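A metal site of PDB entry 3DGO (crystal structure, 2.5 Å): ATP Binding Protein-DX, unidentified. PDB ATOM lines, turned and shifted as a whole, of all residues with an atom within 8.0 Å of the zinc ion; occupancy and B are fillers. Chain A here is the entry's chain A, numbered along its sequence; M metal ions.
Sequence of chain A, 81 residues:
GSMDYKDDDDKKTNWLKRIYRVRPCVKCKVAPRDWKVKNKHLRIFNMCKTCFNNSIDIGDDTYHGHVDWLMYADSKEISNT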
ATOM      1  N   PRO A  24     -26.520  31.703   5.178  1.00  0.00           N
ATOM      2  CA  PRO A  24     -26.167  30.810   6.328  1.00  0.00           C
ATOM      3  C   PRO A  24     -27.148  30.910   7.500  1.00  0.00           C
ATOM      4  O   PRO A  24     -28.065  31.783   7.533  1.00  0.00           O
ATOM      5  CB  PRO A  24     -24.779  31.321   6.767  1.00  0.00           C
ATOM      6  CG  PRO A  24     -24.779  32.769   6.346  1.00  0.00           C
ATOM      7  CD  PRO A  24     -25.579  32.837   5.044  1.00  0.00           C
ATOM      8  N   CYS A  25     -26.968  30.013   8.478  1.00  0.00           N
ATOM      9  CA  CYS A  25     -27.751  30.007   9.689  1.00  0.00           C
ATOM     10  C   CYS A  25     -28.092  31.454  10.137  1.00  0.00           C
ATOM     11  O   CYS A  25     -27.176  32.232  10.389  1.00  0.00           O
ATOM     12  CB  CYS A  25     -26.893  29.313  10.762  1.00  0.00           C
ATOM     13  SG  CYS A  25     -27.677  29.398  12.372  1.00  0.00           S
ATOM     14  N   VAL A  26     -29.371  31.821  10.287  1.00  0.00           N
ATOM     15  CA  VAL A  26     -29.717  33.180  10.780  1.00  0.00           C
ATOM     16  C   VAL A  26     -29.103  33.564  12.144  1.00  0.00           C
ATOM     17  O   VAL A  26     -29.108  34.757  12.497  1.00  0.00           O
ATOM     18  CB  VAL A  26     -31.271  33.455  10.902  1.00  0.00           C
ATOM     19  CG1 VAL A  26     -31.996  33.308   9.573  1.00  0.00           C
ATOM     20  CG2 VAL A  26     -31.894  32.597  12.004  1.00  0.00           C
ATOM     21  N   LYS A  27     -28.599  32.591  12.914  1.00  0.00           N
ATOM     22  CA  LYS A  27     -28.121  32.802  14.300  1.00  0.00           C
ATOM     23  C   LYS A  27     -26.615  32.886  14.426  1.00  0.00           C
ATOM     24  O   LYS A  27     -26.104  33.873  14.942  1.00  0.00           O
ATOM     25  CB  LYS A  27     -28.622  31.711  15.253  1.00  0.00           C
ATOM     26  CG  LYS A  27     -28.133  31.841  16.662  1.00  0.00           C
ATOM     27  CD  LYS A  27     -28.825  32.949  17.424  1.00  0.00           C
ATOM     28  CE  LYS A  27     -28.092  33.168  18.733  1.00  0.00           C
ATOM     29  NZ  LYS A  27     -28.620  34.410  19.369  1.00  0.00           N
ATOM     30  N   CYS A  28     -25.886  31.870  14.001  1.00  0.00           N
ATOM     31  CA  CYS A  28     -24.420  32.003  14.077  1.00  0.00           C
ATOM     32  C   CYS A  28     -23.889  32.719  12.841  1.00  0.00           C
ATOM     33  O   CYS A  28     -22.747  33.063  12.817  1.00  0.00           O
ATOM     34  CB  CYS A  28     -23.735  30.653  14.256  1.00  0.00           C
ATOM     35  SG  CYS A  28     -24.010  29.591  12.790  1.00  0.00           S
ATOM     36  N   LYS A  29     -24.702  32.871  11.796  1.00  0.00           N
ATOM     37  CA  LYS A  29     -24.330  33.654  10.653  1.00  0.00           C
ATOM     38  C   LYS A  29     -23.169  33.042   9.854  1.00  0.00           C
ATOM     39  O   LYS A  29     -22.702  33.650   8.907  1.00  0.00           O
ATOM     40  CB  LYS A  29     -23.958  35.065  11.143  1.00  0.00           C
ATOM     41  CG  LYS A  29     -25.129  35.927  11.743  1.00  0.00           C
ATOM     42  CD  LYS A  29     -25.961  36.560  10.620  1.00  0.00           C
ATOM     43  CE  LYS A  29     -27.186  37.260  11.231  1.00  0.00           C
ATOM     44  NZ  LYS A  29     -26.642  37.650  12.575  1.00  0.00           N
ATOM     45  N   VAL A  30     -22.691  31.864  10.214  1.00  0.00           N
ATOM     46  CA  VAL A  30     -21.563  31.197   9.501  1.00  0.00           C
ATOM     47  C   VAL A  30     -21.880  29.777   8.976  1.00  0.00           C
ATOM     48  O   VAL A  30     -21.701  29.512   7.774  1.00  0.00           O
ATOM     49  CB  VAL A  30     -20.278  31.111  10.379  1.00  0.00           C
ATOM     50  CG1 VAL A  30     -19.168  30.438   9.573  1.00  0.00           C
ATOM     51  CG2 VAL A  30     -19.817  32.502  10.715  1.00  0.00           C
ATOM     52  N   ALA A  31     -22.307  28.854   9.847  1.00  0.00           N
ATOM     53  CA  ALA A  31     -22.735  27.498   9.436  1.00  0.00           C
ATOM     54  C   ALA A  31     -23.952  27.567   8.497  1.00  0.00           C
ATOM     55  O   ALA A  31     -24.797  28.475   8.588  1.00  0.00           O
ATOM     56  CB  ALA A  31     -23.058  26.620  10.652  1.00  0.00           C
ATOM     57  N   PRO A  32     -24.011  26.622   7.540  1.00  0.00           N
ATOM     58  CA  PRO A  32     -25.173  26.578   6.637  1.00  0.00           C
ATOM     59  C   PRO A  32     -26.384  25.988   7.349  1.00  0.00           C
ATOM     60  O   PRO A  32     -26.256  25.376   8.406  1.00  0.00           O
ATOM     61  CB  PRO A  32     -24.673  25.662   5.511  1.00  0.00           C
ATOM     62  CG  PRO A  32     -23.651  24.802   6.139  1.00  0.00           C
ATOM     63  CD  PRO A  32     -22.939  25.699   7.093  1.00  0.00           C
ATOM     64  N   ARG A  33     -27.571  26.172   6.790  1.00  0.00           N
ATOM     65  CA  ARG A  33     -28.793  25.812   7.509  1.00  0.00           C
ATOM     66  C   ARG A  33     -29.053  24.301   7.517  1.00  0.00           C
ATOM     67  O   ARG A  33     -28.635  23.574   6.574  1.00  0.00           O
ATOM     68  CB  ARG A  33     -29.964  26.545   6.905  1.00  0.00           C
ATOM     69  CG  ARG A  33     -29.943  28.013   7.247  1.00  0.00           C
ATOM     70  CD  ARG A  33     -30.935  28.769   6.422  1.00  0.00           C
ATOM     71  NE  ARG A  33     -30.570  30.176   6.450  1.00  0.00           N
ATOM     72  CZ  ARG A  33     -31.414  31.189   6.254  1.00  0.00           C
ATOM     73  NH1 ARG A  33     -32.728  30.968   6.007  1.00  0.00           N
ATOM     74  NH2 ARG A  33     -30.944  32.423   6.304  1.00  0.00           N
ATOM     75  N   ASP A  34     -29.763  23.830   8.550  1.00  0.00           N
ATOM     76  CA  ASP A  34     -30.349  22.550   8.470  1.00  0.00           C
ATOM     77  C   ASP A  34     -31.433  22.517   7.387  1.00  0.00           C
ATOM     78  O   ASP A  34     -31.942  23.552   6.970  1.00  0.00           O
ATOM     79  CB  ASP A  34     -30.958  22.178   9.798  1.00  0.00           C
ATOM     80  CG  ASP A  34     -31.039  20.642   9.976  1.00  0.00           C
ATOM     81  OD1 ASP A  34     -30.571  19.871   9.108  1.00  0.00           O
ATOM     82  OD2 ASP A  34     -31.526  20.194  11.010  1.00  0.00           O
ATOM     83  N   ASN A  46     -34.272  27.600   9.515  1.00  0.00           N
ATOM     84  CA  ASN A  46     -33.571  28.866   9.678  1.00  0.00           C
ATOM     85  C   ASN A  46     -32.141  28.790  10.264  1.00  0.00           C
ATOM     86  O   ASN A  46     -31.291  29.694   9.993  1.00  0.00           O
ATOM     87  CB  ASN A  46     -34.446  29.832  10.472  1.00  0.00           C
ATOM     88  CG  ASN A  46     -35.721  30.213   9.718  1.00  0.00           C
ATOM     89  OD1 ASN A  46     -35.841  30.035   8.472  1.00  0.00           O
ATOM     90  ND2 ASN A  46     -36.671  30.738  10.448  1.00  0.00           N
ATOM     91  N   MET A  47     -31.899  27.720  11.040  1.00  0.00           N
ATOM     92  CA  MET A  47     -30.665  27.519  11.731  1.00  0.00           C
ATOM     93  C   MET A  47     -29.986  26.203  11.425  1.00  0.00           C
ATOM     94  O   MET A  47     -30.652  25.223  11.006  1.00  0.00           O
ATOM     95  CB  MET A  47     -30.915  27.592  13.214  1.00  0.00           C
ATOM     96  CG  MET A  47     -31.318  28.969  13.672  1.00  0.00           C
ATOM     97  SD  MET A  47     -31.490  29.020  15.509  1.00  0.00           S
ATOM     98  CE  MET A  47     -33.019  28.091  15.832  1.00  0.00           C
ATOM     99  N   CYS A  48     -28.667  26.159  11.636  1.00  0.00           N
ATOM    100  CA  CYS A  48     -27.949  24.867  11.573  1.00  0.00           C
ATOM    101  C   CYS A  48     -28.456  23.976  12.746  1.00  0.00           C
ATOM    102  O   CYS A  48     -29.203  24.455  13.656  1.00  0.00           O
ATOM    103  CB  CYS A  48     -26.405  25.082  11.600  1.00  0.00           C
ATOM    104  SG  CYS A  48     -25.861  25.773  13.124  1.00  0.00           S
ATOM    105  N   LYS A  49     -28.090  22.685  12.765  1.00  0.00           N
ATOM    106  CA  LYS A  49     -28.635  21.879  13.864  1.00  0.00           C
ATOM    107  C   LYS A  49     -28.082  22.302  15.266  1.00  0.00           C
ATOM    108  O   LYS A  49     -28.852  22.270  16.270  1.00  0.00           O
ATOM    109  CB  LYS A  49     -28.524  20.354  13.615  1.00  0.00           C
ATOM    110  CG  LYS A  49     -28.929  19.568  14.849  1.00  0.00           C
ATOM    111  CD  LYS A  49     -29.442  18.194  14.569  1.00  0.00           C
ATOM    112  CE  LYS A  49     -30.668  18.308  13.608  1.00  0.00           C
ATOM    113  NZ  LYS A  49     -31.858  18.985  14.210  1.00  0.00           N
ATOM    114  N   THR A  50     -26.822  22.728  15.325  1.00  0.00           N
ATOM    115  CA  THR A  50     -26.201  23.077  16.563  1.00  0.00           C
ATOM    116  C   THR A  50     -26.863  24.292  17.188  1.00  0.00           C
ATOM    117  O   THR A  50     -27.201  24.272  18.378  1.00  0.00           O
ATOM    118  CB  THR A  50     -24.711  23.388  16.349  1.00  0.00           C
ATOM    119  OG1 THR A  50     -24.051  22.212  15.863  1.00  0.00           O
ATOM    120  CG2 THR A  50     -24.032  23.742  17.672  1.00  0.00           C
ATOM    121  N   CYS A  51     -27.047  25.369  16.419  1.00  0.00           N
ATOM    122  CA  CYS A  51     -27.746  26.531  16.962  1.00  0.00           C
ATOM    123  C   CYS A  51     -29.188  26.217  17.313  1.00  0.00           C
ATOM    124  O   CYS A  51     -29.697  26.755  18.296  1.00  0.00           O
ATOM    125  CB  CYS A  51     -27.747  27.671  15.983  1.00  0.00           C
ATOM    126  SG  CYS A  51     -26.116  28.419  15.825  1.00  0.00           S
ATOM    127  N   PHE A  52     -29.866  25.376  16.526  1.00  0.00           N
ATOM    128  CA  PHE A  52     -31.237  24.992  16.865  1.00  0.00           C
ATOM    129  C   PHE A  52     -31.310  24.264  18.237  1.00  0.00           C
ATOM    130  O   PHE A  52     -32.067  24.676  19.150  1.00  0.00           O
ATOM    131  CB  PHE A  52     -31.882  24.159  15.754  1.00  0.00           C
ATOM    132  CG  PHE A  52     -33.269  23.730  16.079  1.00  0.00           C
ATOM    133  CD1 PHE A  52     -34.329  24.666  16.100  1.00  0.00           C
ATOM    134  CD2 PHE A  52     -33.541  22.376  16.398  1.00  0.00           C
ATOM    135  CE1 PHE A  52     -35.659  24.280  16.431  1.00  0.00           C
ATOM    136  CE2 PHE A  52     -34.885  21.972  16.723  1.00  0.00           C
ATOM    137  CZ  PHE A  52     -35.938  22.943  16.749  1.00  0.00           C
HETATM  138 ZN    ZN M   1     -25.903  28.408  13.466  1.00  0.00          ZN
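SG of Cys 25 sits close to N of Lys 27, at 3.4 Å.
The side-chain sulfur (SG) of Cys 28 sits close to the backbone NH (N) of Val 30 (3.7 Å).
The backbone NH of Cys 25 is in hydrogen-bond range of the backbone carbonyl oxygen of Ala 31 (2.7 Å).
The backbone NH (N) of Ala 31 lies close to the side-chain sulfur (SG) of Cys 28 (3.5 Å).
Within 4 Å of the zinc ion: Cys 25, Cys 28, Cys 48 and Cys 51.
The nearest printed residue that does not touch the zinc ion is Ala 31 (4.4 Å).
The zinc ion is bound by SG of Cys 25 (2.3 Å), SG of Cys 28 (2.3 Å), SG of Cys 51 (2.4 Å) and SG of Cys 48 (2.7 Å).
The zinc ion has four donor atoms within binding distance.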
